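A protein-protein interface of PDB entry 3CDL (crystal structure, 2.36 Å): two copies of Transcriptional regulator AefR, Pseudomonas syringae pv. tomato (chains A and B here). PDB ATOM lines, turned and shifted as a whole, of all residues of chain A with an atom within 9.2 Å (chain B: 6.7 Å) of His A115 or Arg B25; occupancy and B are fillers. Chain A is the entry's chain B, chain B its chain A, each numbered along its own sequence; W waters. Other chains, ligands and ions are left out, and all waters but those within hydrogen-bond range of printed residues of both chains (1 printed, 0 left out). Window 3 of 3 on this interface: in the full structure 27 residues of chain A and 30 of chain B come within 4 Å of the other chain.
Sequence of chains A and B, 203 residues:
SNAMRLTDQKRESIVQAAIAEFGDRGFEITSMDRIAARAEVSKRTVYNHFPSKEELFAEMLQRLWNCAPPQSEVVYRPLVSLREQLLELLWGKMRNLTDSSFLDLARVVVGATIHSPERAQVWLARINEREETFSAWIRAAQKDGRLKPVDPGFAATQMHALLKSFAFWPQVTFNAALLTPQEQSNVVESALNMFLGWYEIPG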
ATOM      1  N   GLU A  28     -22.987  23.928   0.267  1.00  0.00           N
ATOM      2  CA  GLU A  28     -22.425  25.273   0.023  1.00  0.00           C
ATOM      3  C   GLU A  28     -21.817  25.468  -1.356  1.00  0.00           C
ATOM      4  O   GLU A  28     -21.925  26.557  -1.917  1.00  0.00           O
ATOM      5  CB  GLU A  28     -21.423  25.688   1.115  1.00  0.00           C
ATOM      6  CG  GLU A  28     -22.023  26.539   2.286  1.00  0.00           C
ATOM      7  CD  GLU A  28     -22.239  28.049   1.936  1.00  0.00           C
ATOM      8  OE1 GLU A  28     -22.715  28.373   0.820  1.00  0.00           O
ATOM      9  OE2 GLU A  28     -21.946  28.920   2.794  1.00  0.00           O
ATOM     10  N   VAL A 108     -29.325  14.943   3.648  1.00  0.00           N
ATOM     11  CA  VAL A 108     -28.810  16.239   3.210  1.00  0.00           C
ATOM     12  C   VAL A 108     -28.969  17.342   4.275  1.00  0.00           C
ATOM     13  O   VAL A 108     -28.083  18.165   4.386  1.00  0.00           O
ATOM     14  CB  VAL A 108     -29.179  16.664   1.718  1.00  0.00           C
ATOM     15  CG1 VAL A 108     -29.421  15.453   0.843  1.00  0.00           C
ATOM     16  CG2 VAL A 108     -30.339  17.597   1.647  1.00  0.00           C
ATOM     17  N   VAL A 109     -30.040  17.330   5.078  1.00  0.00           N
ATOM     18  CA  VAL A 109     -30.241  18.409   6.072  1.00  0.00           C
ATOM     19  C   VAL A 109     -29.280  18.312   7.262  1.00  0.00           C
ATOM     20  O   VAL A 109     -28.642  19.296   7.646  1.00  0.00           O
ATOM     21  CB  VAL A 109     -31.727  18.542   6.561  1.00  0.00           C
ATOM     22  CG1 VAL A 109     -31.849  19.600   7.627  1.00  0.00           C
ATOM     23  CG2 VAL A 109     -32.623  18.921   5.413  1.00  0.00           C
ATOM     24  N   VAL A 110     -29.197  17.115   7.835  1.00  0.00           N
ATOM     25  CA  VAL A 110     -28.162  16.783   8.790  1.00  0.00           C
ATOM     26  C   VAL A 110     -26.769  17.040   8.229  1.00  0.00           C
ATOM     27  O   VAL A 110     -25.915  17.625   8.901  1.00  0.00           O
ATOM     28  CB  VAL A 110     -28.278  15.319   9.247  1.00  0.00           C
ATOM     29  CG1 VAL A 110     -27.139  14.977  10.236  1.00  0.00           C
ATOM     30  CG2 VAL A 110     -29.642  15.087   9.878  1.00  0.00           C
ATOM     31  N   GLY A 111     -26.538  16.602   6.999  1.00  0.00           N
ATOM     32  CA  GLY A 111     -25.259  16.848   6.348  1.00  0.00           C
ATOM     33  C   GLY A 111     -24.965  18.329   6.205  1.00  0.00           C
ATOM     34  O   GLY A 111     -23.810  18.764   6.295  1.00  0.00           O
ATOM     35  N   ALA A 112     -26.010  19.112   5.983  1.00  0.00           N
ATOM     36  CA  ALA A 112     -25.817  20.531   5.807  1.00  0.00           C
ATOM     37  C   ALA A 112     -25.667  21.250   7.144  1.00  0.00           C
ATOM     38  O   ALA A 112     -25.115  22.333   7.193  1.00  0.00           O
ATOM     39  CB  ALA A 112     -26.951  21.152   4.944  1.00  0.00           C
ATOM     40  N   THR A 113     -26.157  20.682   8.239  1.00  0.00           N
ATOM     41  CA  THR A 113     -26.019  21.432   9.499  1.00  0.00           C
ATOM     42  C   THR A 113     -24.844  21.009  10.360  1.00  0.00           C
ATOM     43  O   THR A 113     -24.334  21.821  11.119  1.00  0.00           O
ATOM     44  CB  THR A 113     -27.356  21.567  10.347  1.00  0.00           C
ATOM     45  OG1 THR A 113     -27.446  20.523  11.316  1.00  0.00           O
ATOM     46  CG2 THR A 113     -28.571  21.520   9.478  1.00  0.00           C
ATOM     47  N   ILE A 114     -24.412  19.757  10.222  1.00  0.00           N
ATOM     48  CA  ILE A 114     -23.416  19.159  11.138  1.00  0.00           C
ATOM     49  C   ILE A 114     -22.155  20.012  11.342  1.00  0.00           C
ATOM     50  O   ILE A 114     -21.776  20.314  12.498  1.00  0.00           O
ATOM     51  CB  ILE A 114     -23.081  17.665  10.786  1.00  0.00           C
ATOM     52  CG1 ILE A 114     -22.160  17.033  11.848  1.00  0.00           C
ATOM     53  CG2 ILE A 114     -22.531  17.517   9.355  1.00  0.00           C
ATOM     54  CD1 ILE A 114     -22.394  15.526  12.071  1.00  0.00           C
ATOM     55  N   HIS A 115     -21.533  20.422  10.237  1.00  0.00           N
ATOM     56  CA  HIS A 115     -20.339  21.284  10.320  1.00  0.00           C
ATOM     57  C   HIS A 115     -20.594  22.741   9.929  1.00  0.00           C
ATOM     58  O   HIS A 115     -19.709  23.408   9.438  1.00  0.00           O
ATOM     59  CB  HIS A 115     -19.153  20.672   9.541  1.00  0.00           C
ATOM     60  CG  HIS A 115     -18.631  19.418  10.167  1.00  0.00           C
ATOM     61  ND1 HIS A 115     -17.853  19.423  11.312  1.00  0.00           N
ATOM     62  CD2 HIS A 115     -18.815  18.116   9.841  1.00  0.00           C
ATOM     63  CE1 HIS A 115     -17.565  18.179  11.649  1.00  0.00           C
ATOM     64  NE2 HIS A 115     -18.143  17.365  10.775  1.00  0.00           N
ATOM     65  N   SER A 116     -21.814  23.213  10.150  1.00  0.00           N
ATOM     66  CA  SER A 116     -22.217  24.564   9.782  1.00  0.00           C
ATOM     67  C   SER A 116     -22.928  25.248  10.944  1.00  0.00           C
ATOM     68  O   SER A 116     -24.147  25.086  11.112  1.00  0.00           O
ATOM     69  CB  SER A 116     -23.153  24.534   8.587  1.00  0.00           C
ATOM     70  OG  SER A 116     -23.910  25.738   8.544  1.00  0.00           O
ATOM     71  N   PRO A 117     -22.177  26.042  11.725  1.00  0.00           N
ATOM     72  CA  PRO A 117     -22.677  26.749  12.899  1.00  0.00           C
ATOM     73  C   PRO A 117     -23.962  27.551  12.648  1.00  0.00           C
ATOM     74  O   PRO A 117     -24.917  27.380  13.380  1.00  0.00           O
ATOM     75  CB  PRO A 117     -21.513  27.684  13.257  1.00  0.00           C
ATOM     76  CG  PRO A 117     -20.300  26.991  12.734  1.00  0.00           C
ATOM     77  CD  PRO A 117     -20.747  26.326  11.479  1.00  0.00           C
ATOM     78  N   GLU A 118     -23.974  28.408  11.629  1.00  0.00           N
ATOM     79  CA  GLU A 118     -25.143  29.231  11.254  1.00  0.00           C
ATOM     80  C   GLU A 118     -26.378  28.416  10.929  1.00  0.00           C
ATOM     81  O   GLU A 118     -27.504  28.846  11.153  1.00  0.00           O
ATOM     82  CB  GLU A 118     -24.800  30.073  10.022  1.00  0.00           C
ATOM     83  CG  GLU A 118     -25.994  30.694   9.267  1.00  0.00           C
ATOM     84  CD  GLU A 118     -25.580  31.881   8.402  1.00  0.00           C
ATOM     85  OE1 GLU A 118     -25.842  31.835   7.174  1.00  0.00           O
ATOM     86  OE2 GLU A 118     -24.986  32.849   8.944  1.00  0.00           O
ATOM     87  N   ARG A 119     -26.150  27.252  10.352  1.00  0.00           N
ATOM     88  CA  ARG A 119     -27.212  26.387   9.943  1.00  0.00           C
ATOM     89  C   ARG A 119     -27.671  25.610  11.189  1.00  0.00           C
ATOM     90  O   ARG A 119     -28.853  25.265  11.318  1.00  0.00           O
ATOM     91  CB  ARG A 119     -26.672  25.460   8.873  1.00  0.00           C
ATOM     92  CG  ARG A 119     -27.592  25.150   7.720  1.00  0.00           C
ATOM     93  CD  ARG A 119     -27.571  26.123   6.548  1.00  0.00           C
ATOM     94  NE  ARG A 119     -26.260  26.364   5.925  1.00  0.00           N
ATOM     95  CZ  ARG A 119     -25.425  25.418   5.499  1.00  0.00           C
ATOM     96  NH1 ARG A 119     -25.746  24.148   5.659  1.00  0.00           N
ATOM     97  NH2 ARG A 119     -24.263  25.738   4.946  1.00  0.00           N
ATOM     98  N   ALA A 120     -26.741  25.350  12.111  1.00  0.00           N
ATOM     99  CA  ALA A 120     -27.080  24.720  13.387  1.00  0.00           C
ATOM    100  C   ALA A 120     -28.006  25.622  14.193  1.00  0.00           C
ATOM    101  O   ALA A 120     -28.978  25.163  14.754  1.00  0.00           O
ATOM    102  CB  ALA A 120     -25.841  24.400  14.175  1.00  0.00           C
ATOM    103  N   ALA B  20      -7.729  18.881  15.204  1.00  0.00           N
ATOM    104  CA  ALA B  20      -8.137  20.282  15.314  1.00  0.00           C
ATOM    105  C   ALA B  20      -8.869  20.758  14.044  1.00  0.00           C
ATOM    106  O   ALA B  20      -9.933  21.352  14.135  1.00  0.00           O
ATOM    107  CB  ALA B  20      -6.930  21.191  15.646  1.00  0.00           C
ATOM    108  N   GLU B  21      -8.326  20.463  12.859  1.00  0.00           N
ATOM    109  CA  GLU B  21      -8.904  20.986  11.614  1.00  0.00           C
ATOM    110  C   GLU B  21     -10.220  20.323  11.228  1.00  0.00           C
ATOM    111  O   GLU B  21     -11.223  21.016  10.942  1.00  0.00           O
ATOM    112  CB  GLU B  21      -7.902  20.930  10.467  1.00  0.00           C
ATOM    113  CG  GLU B  21      -6.703  21.846  10.638  1.00  0.00           C
ATOM    114  CD  GLU B  21      -7.057  23.305  10.502  1.00  0.00           C
ATOM    115  OE1 GLU B  21      -8.146  23.629   9.967  1.00  0.00           O
ATOM    116  OE2 GLU B  21      -6.237  24.146  10.922  1.00  0.00           O
ATOM    117  N   PHE B  22     -10.211  18.990  11.220  1.00  0.00           N
ATOM    118  CA  PHE B  22     -11.428  18.195  11.098  1.00  0.00           C
ATOM    119  C   PHE B  22     -12.530  18.641  12.119  1.00  0.00           C
ATOM    120  O   PHE B  22     -13.674  18.937  11.744  1.00  0.00           O
ATOM    121  CB  PHE B  22     -11.102  16.699  11.276  1.00  0.00           C
ATOM    122  CG  PHE B  22     -10.300  16.063  10.128  1.00  0.00           C
ATOM    123  CD1 PHE B  22      -9.583  14.884  10.351  1.00  0.00           C
ATOM    124  CD2 PHE B  22     -10.297  16.595   8.848  1.00  0.00           C
ATOM    125  CE1 PHE B  22      -8.864  14.251   9.322  1.00  0.00           C
ATOM    126  CE2 PHE B  22      -9.579  15.980   7.812  1.00  0.00           C
ATOM    127  CZ  PHE B  22      -8.863  14.807   8.050  1.00  0.00           C
ATOM    128  N   GLY B  23     -12.176  18.695  13.410  1.00  0.00           N
ATOM    129  CA  GLY B  23     -13.119  19.114  14.457  1.00  0.00           C
ATOM    130  C   GLY B  23     -13.814  20.441  14.156  1.00  0.00           C
ATOM    131  O   GLY B  23     -15.019  20.595  14.444  1.00  0.00           O
ATOM    132  N   ASP B  24     -13.052  21.384  13.579  1.00  0.00           N
ATOM    133  CA  ASP B  24     -13.540  22.707  13.193  1.00  0.00           C
ATOM    134  C   ASP B  24     -14.429  22.759  11.948  1.00  0.00           C
ATOM    135  O   ASP B  24     -15.574  23.205  12.038  1.00  0.00           O
ATOM    136  CB  ASP B  24     -12.360  23.652  12.988  1.00  0.00           C
ATOM    137  CG  ASP B  24     -11.684  24.027  14.300  1.00  0.00           C
ATOM    138  OD1 ASP B  24     -12.395  24.049  15.344  1.00  0.00           O
ATOM    139  OD2 ASP B  24     -10.448  24.306  14.281  1.00  0.00           O
ATOM    140  N   ARG B  25     -13.914  22.327  10.798  1.00  0.00           N
ATOM    141  CA  ARG B  25     -14.655  22.447   9.538  1.00  0.00           C
ATOM    142  C   ARG B  25     -15.201  21.132   8.935  1.00  0.00           C
ATOM    143  O   ARG B  25     -15.805  21.136   7.865  1.00  0.00           O
ATOM    144  CB  ARG B  25     -13.807  23.192   8.495  1.00  0.00           C
ATOM    145  CG  ARG B  25     -13.226  24.545   8.949  1.00  0.00           C
ATOM    146  CD  ARG B  25     -12.638  25.395   7.793  1.00  0.00           C
ATOM    147  NE  ARG B  25     -11.724  24.601   6.981  1.00  0.00           N
ATOM    148  CZ  ARG B  25     -11.736  24.553   5.653  1.00  0.00           C
ATOM    149  NH1 ARG B  25     -12.579  25.313   4.955  1.00  0.00           N
ATOM    150  NH2 ARG B  25     -10.859  23.770   5.017  1.00  0.00           N
ATOM    151  N   GLY B  26     -14.990  20.009   9.603  1.00  0.00           N
ATOM    152  CA  GLY B  26     -15.396  18.717   9.077  1.00  0.00           C
ATOM    153  C   GLY B  26     -14.296  17.987   8.323  1.00  0.00           C
ATOM    154  O   GLY B  26     -13.307  18.571   7.893  1.00  0.00           O
ATOM    155  N   PHE B  27     -14.506  16.694   8.141  1.00  0.00           N
ATOM    156  CA  PHE B  27     -13.555  15.818   7.519  1.00  0.00           C
ATOM    157  C   PHE B  27     -13.351  16.133   6.040  1.00  0.00           C
ATOM    158  O   PHE B  27     -12.214  16.216   5.604  1.00  0.00           O
ATOM    159  CB  PHE B  27     -14.022  14.365   7.685  1.00  0.00           C
ATOM    160  CG  PHE B  27     -13.118  13.355   7.045  1.00  0.00           C
ATOM    161  CD1 PHE B  27     -11.992  12.892   7.712  1.00  0.00           C
ATOM    162  CD2 PHE B  27     -13.392  12.871   5.774  1.00  0.00           C
ATOM    163  CE1 PHE B  27     -11.136  11.954   7.117  1.00  0.00           C
ATOM    164  CE2 PHE B  27     -12.559  11.930   5.174  1.00  0.00           C
ATOM    165  CZ  PHE B  27     -11.418  11.470   5.853  1.00  0.00           C
ATOM    166  N   GLU B  28     -14.445  16.313   5.293  1.00  0.00           N
ATOM    167  CA  GLU B  28     -14.424  16.363   3.824  1.00  0.00           C
ATOM    168  C   GLU B  28     -13.770  17.614   3.232  1.00  0.00           C
ATOM    169  O   GLU B  28     -12.965  17.544   2.310  1.00  0.00           O
ATOM    170  CB  GLU B  28     -15.852  16.215   3.294  1.00  0.00           C
ATOM    171  CG  GLU B  28     -16.451  14.803   3.442  1.00  0.00           C
ATOM    172  CD  GLU B  28     -16.084  13.877   2.278  1.00  0.00           C
ATOM    173  OE1 GLU B  28     -16.229  12.650   2.449  1.00  0.00           O
ATOM    174  OE2 GLU B  28     -15.646  14.352   1.198  1.00  0.00           O
ATOM    175  N   ILE B  29     -14.139  18.756   3.796  1.00  0.00           N
ATOM    176  CA  ILE B  29     -13.688  20.082   3.387  1.00  0.00           C
ATOM    177  C   ILE B  29     -12.260  20.317   3.833  1.00  0.00           C
ATOM    178  O   ILE B  29     -11.566  21.134   3.232  1.00  0.00           O
ATOM    179  CB  ILE B  29     -14.631  21.169   3.996  1.00  0.00           C
ATOM    180  CG1 ILE B  29     -14.517  22.520   3.277  1.00  0.00           C
ATOM    181  CG2 ILE B  29     -14.413  21.307   5.486  1.00  0.00           C
ATOM    182  CD1 ILE B  29     -15.685  23.492   3.611  1.00  0.00           C
ATOM    183  N   THR B  30     -11.819  19.629   4.887  1.00  0.00           N
ATOM    184  CA  THR B  30     -10.408  19.692   5.283  1.00  0.00           C
ATOM    185  C   THR B  30      -9.578  18.885   4.277  1.00  0.00           C
ATOM    186  O   THR B  30      -9.868  17.705   4.014  1.00  0.00           O
ATOM    187  CB  THR B  30     -10.145  19.209   6.736  1.00  0.00           C
ATOM    188  OG1 THR B  30     -11.029  19.865   7.641  1.00  0.00           O
ATOM    189  CG2 THR B  30      -8.732  19.540   7.173  1.00  0.00           C
ATOM    190  N   SER B  31      -8.575  19.549   3.701  1.00  0.00           N
ATOM    191  CA  SER B  31      -7.666  18.962   2.740  1.00  0.00           C
ATOM    192  C   SER B  31      -6.304  18.796   3.370  1.00  0.00           C
ATOM    193  O   SER B  31      -5.984  19.447   4.361  1.00  0.00           O
ATOM    194  CB  SER B  31      -7.507  19.893   1.543  1.00  0.00           C
ATOM    195  OG  SER B  31      -6.764  21.047   1.926  1.00  0.00           O
ATOM    196  N   ARG B  34      -3.866  21.642   4.054  1.00  0.00           N
ATOM    197  CA  ARG B  34      -4.440  22.441   5.133  1.00  0.00           C
ATOM    198  C   ARG B  34      -4.019  21.863   6.478  1.00  0.00           C
ATOM    199  O   ARG B  34      -3.643  22.591   7.395  1.00  0.00           O
ATOM    200  CB  ARG B  34      -5.961  22.494   5.034  1.00  0.00           C
ATOM    201  CG  ARG B  34      -6.639  22.957   6.294  1.00  0.00           C
ATOM    202  CD  ARG B  34      -6.554  24.454   6.406  1.00  0.00           C
ATOM    203  NE  ARG B  34      -7.531  25.016   7.340  1.00  0.00           N
ATOM    204  CZ  ARG B  34      -8.476  25.898   7.031  1.00  0.00           C
ATOM    205  NH1 ARG B  34      -9.286  26.341   7.980  1.00  0.00           N
ATOM    206  NH2 ARG B  34      -8.608  26.359   5.794  1.00  0.00           N
ATOM    207  N   ASP B 104     -16.346  16.410  19.555  1.00  0.00           N
ATOM    208  CA  ASP B 104     -15.753  16.943  18.335  1.00  0.00           C
ATOM    209  C   ASP B 104     -15.311  15.806  17.454  1.00  0.00           C
ATOM    210  O   ASP B 104     -15.681  15.738  16.297  1.00  0.00           O
ATOM    211  CB  ASP B 104     -14.575  17.838  18.655  1.00  0.00           C
ATOM    212  CG  ASP B 104     -14.991  19.184  19.158  1.00  0.00           C
ATOM    213  OD1 ASP B 104     -16.185  19.369  19.431  1.00  0.00           O
ATOM    214  OD2 ASP B 104     -14.112  20.055  19.302  1.00  0.00           O
ATOM    215  N   ARG B 107     -18.174  14.069  16.122  1.00  0.00           N
ATOM    216  CA  ARG B 107     -18.780  14.851  15.027  1.00  0.00           C
ATOM    217  C   ARG B 107     -18.074  14.674  13.692  1.00  0.00           C
ATOM    218  O   ARG B 107     -18.755  14.508  12.670  1.00  0.00           O
ATOM    219  CB  ARG B 107     -18.882  16.349  15.385  1.00  0.00           C
ATOM    220  CG  ARG B 107     -19.862  17.185  14.503  1.00  0.00           C
ATOM    221  CD  ARG B 107     -20.312  18.489  15.214  1.00  0.00           C
ATOM    222  NE  ARG B 107     -19.265  18.853  16.158  1.00  0.00           N
ATOM    223  CZ  ARG B 107     -19.426  19.083  17.450  1.00  0.00           C
ATOM    224  NH1 ARG B 107     -20.632  19.127  17.992  1.00  0.00           N
ATOM    225  NH2 ARG B 107     -18.352  19.335  18.188  1.00  0.00           N
ATOM    226  N   VAL B 108     -16.727  14.742  13.679  1.00  0.00           N
ATOM    227  CA  VAL B 108     -16.001  14.545  12.415  1.00  0.00           C
ATOM    228  C   VAL B 108     -16.383  13.188  11.808  1.00  0.00           C
ATOM    229  O   VAL B 108     -16.677  13.089  10.603  1.00  0.00           O
ATOM    230  CB  VAL B 108     -14.406  14.834  12.416  1.00  0.00           C
ATOM    231  CG1 VAL B 108     -13.833  15.312  13.742  1.00  0.00           C
ATOM    232  CG2 VAL B 108     -13.583  13.663  11.795  1.00  0.00           C
ATOM    233  N   VAL B 109     -16.384  12.163  12.650  1.00  0.00           N
ATOM    234  CA  VAL B 109     -16.702  10.793  12.254  1.00  0.00           C
ATOM    235  C   VAL B 109     -18.138  10.614  11.711  1.00  0.00           C
ATOM    236  O   VAL B 109     -18.327   9.974  10.649  1.00  0.00           O
ATOM    237  CB  VAL B 109     -16.408   9.823  13.433  1.00  0.00           C
ATOM    238  CG1 VAL B 109     -17.132   8.488  13.279  1.00  0.00           C
ATOM    239  CG2 VAL B 109     -14.917   9.617  13.558  1.00  0.00           C
ATOM    240  N   VAL B 110     -19.132  11.154  12.440  1.00  0.00           N
ATOM    241  CA  VAL B 110     -20.513  11.154  11.962  1.00  0.00           C
ATOM    242  C   VAL B 110     -20.609  11.907  10.629  1.00  0.00           C
ATOM    243  O   VAL B 110     -21.267  11.439   9.688  1.00  0.00           O
ATOM    244  CB  VAL B 110     -21.548  11.744  12.988  1.00  0.00           C
ATOM    245  CG1 VAL B 110     -22.952  11.703  12.399  1.00  0.00           C
ATOM    246  CG2 VAL B 110     -21.548  10.988  14.329  1.00  0.00           C
ATOM    247  N   GLY B 111     -19.946  13.060  10.532  1.00  0.00           N
ATOM    248  CA  GLY B 111     -20.017  13.866   9.311  1.00  0.00           C
ATOM    249  C   GLY B 111     -19.358  13.203   8.117  1.00  0.00           C
ATOM    250  O   GLY B 111     -19.789  13.384   6.957  1.00  0.00           O
ATOM    251  N   ALA B 112     -18.306  12.433   8.382  1.00  0.00           N
ATOM    252  CA  ALA B 112     -17.543  11.821   7.317  1.00  0.00           C
ATOM    253  C   ALA B 112     -18.278  10.635   6.665  1.00  0.00           C
ATOM    254  O   ALA B 112     -17.950  10.225   5.547  1.00  0.00           O
ATOM    255  CB  ALA B 112     -16.184  11.390   7.857  1.00  0.00           C
ATOM    256  N   HIS B 115     -21.475  12.342   4.624  1.00  0.00           N
ATOM    257  CA  HIS B 115     -20.905  12.997   3.449  1.00  0.00           C
ATOM    258  C   HIS B 115     -20.315  11.959   2.472  1.00  0.00           C
ATOM    259  O   HIS B 115     -20.146  12.261   1.286  1.00  0.00           O
ATOM    260  CB  HIS B 115     -19.884  14.105   3.809  1.00  0.00           C
ATOM    261  CG  HIS B 115     -20.449  15.244   4.629  1.00  0.00           C
ATOM    262  ND1 HIS B 115     -19.653  16.108   5.358  1.00  0.00           N
ATOM    263  CD2 HIS B 115     -21.725  15.661   4.834  1.00  0.00           C
ATOM    264  CE1 HIS B 115     -20.412  16.999   5.976  1.00  0.00           C
ATOM    265  NE2 HIS B 115     -21.675  16.739   5.689  1.00  0.00           N
ATOM    266  N   VAL B 172     -24.067  16.895  18.336  1.00  0.00           N
ATOM    267  CA  VAL B 172     -23.275  16.489  17.220  1.00  0.00           C
ATOM    268  C   VAL B 172     -23.918  16.969  15.904  1.00  0.00           C
ATOM    269  O   VAL B 172     -23.205  17.379  14.976  1.00  0.00           O
ATOM    270  CB  VAL B 172     -23.102  14.956  17.263  1.00  0.00           C
ATOM    271  CG1 VAL B 172     -22.630  14.387  15.915  1.00  0.00           C
ATOM    272  CG2 VAL B 172     -22.133  14.576  18.372  1.00  0.00           C
ATOM    273  N   THR B 173     -25.249  16.958  15.819  1.00  0.00           N
ATOM    274  CA  THR B 173     -25.895  17.387  14.570  1.00  0.00           C
ATOM    275  C   THR B 173     -26.206  18.880  14.498  1.00  0.00           C
ATOM    276  O   THR B 173     -26.270  19.407  13.395  1.00  0.00           O
ATOM    277  CB  THR B 173     -27.145  16.539  14.197  1.00  0.00           C
ATOM    278  OG1 THR B 173     -28.193  16.811  15.121  1.00  0.00           O
ATOM    279  CG2 THR B 173     -26.821  15.031  14.210  1.00  0.00           C
HETATM  280  O   HOH W   1     -17.569  21.263  13.046  1.00  0.00           O
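OG1 of Thr A113 lies within hydrogen-bond range of O of Thr B173 (2.6 Å).
A ring nitrogen (NE2) of His B115 lies within hydrogen-bond range of the backbone carbonyl oxygen (O) of Gly A111 (3.0 Å).
O of Arg B107 is in hydrogen-bond range of NE2 of His A115, 3.5 Å away.
N of Gly B26 sits at hydrogen-bond distance from ND1 of His A115, at 3.4 Å.
O of Gly B26 is in hydrogen-bond range of OG1 of Thr B30.
The backbone carbonyl oxygen (O) of Ile B29 lies within hydrogen-bond range of the guanidinium group (NH2) of Arg B25.
OD1 of Asp B104 is in salt-bridge range of NH2 of Arg B107, at 2.5 Å.
The backbone carbonyl oxygen (O) of Gly B111 sits close to a ring nitrogen (ND1) of His B115.
Among the printed residues, merely in contact across the chains: Val A110 with Thr B173, Ile A114 with Arg B107, Ile A114 with Val B110, Ile A114 with Gly B111, Ile A114 with His B115, Ile A114 with Val B172, Ile A114 with Thr B173, His A115 with Phe B22, His A115 with Arg B25 and His A115 with Val B108.
Glu A28 touches none of the printed residues of chain B.
Printed residues of chain B within 4 Å of Val A110: Thr B173.
Printed residues of chain B within 4 Å of Gly A111: His B115 (3.0 Å).
Of chain B, only Phe B22, Arg B25, Gly B26, Arg B107 and Val B108 come within 4 Å of His A115.
No residue of chain A comes within 4 Å of Gly B23.
Arg B25 touches just one residue of chain A: His A115.
Gly B26 touches one residue of chain A.
Printed residues of chain A within 4 Å of Val B108: His A115.
The nearest residue of chain B that does not touch His A115 is Gly B111 (4.2 Å).
The nearest residue of chain A that does not touch Arg B25 is Ser A116 (6.8 Å).
The nearest printed residue of chain B that does not touch Thr A113 is Val B172 (6.0 Å).
Of the 14 printed residues of chain A, 5 touch a printed residue of chain B.
Printed residues of chain A that touch a printed residue of chain B: Val A110, Gly A111, Thr A113, Ile A114 and His A115.
Printed residues of chain B that touch a printed residue of chain A: Phe B22, Arg B25, Gly B26, Arg B107, Val B108, Val B110, Gly B111, His B115, Val B172 and Thr B173.
Hydrophobic or aromatic side chains of chain B within 4 Å of the printed part of chain A: Val B110 and His B115.
Among the printed residues, no Asp or Glu carboxylate lies within 4 Å of a Lys or Arg side-chain nitrogen of the other chain.
Gly A111 touches His B115, but with the chains exchanged His A115 does not touch Gly B111 (4.2 Å).
His A115 touches Val B108, but with the chains exchanged Val A108 does not touch His B115 (6.7 Å).
7 positions are printed for both chains.
Of the 14 pairs that touch across the chains among the printed residues, none has its exchanged pair printed and touching as well.
Water W1 lies within hydrogen-bond range of ND1 of His A115 (2.5 Å), O of Asp B24 (3.0 Å) and O of Gly B23 (3.0 Å).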
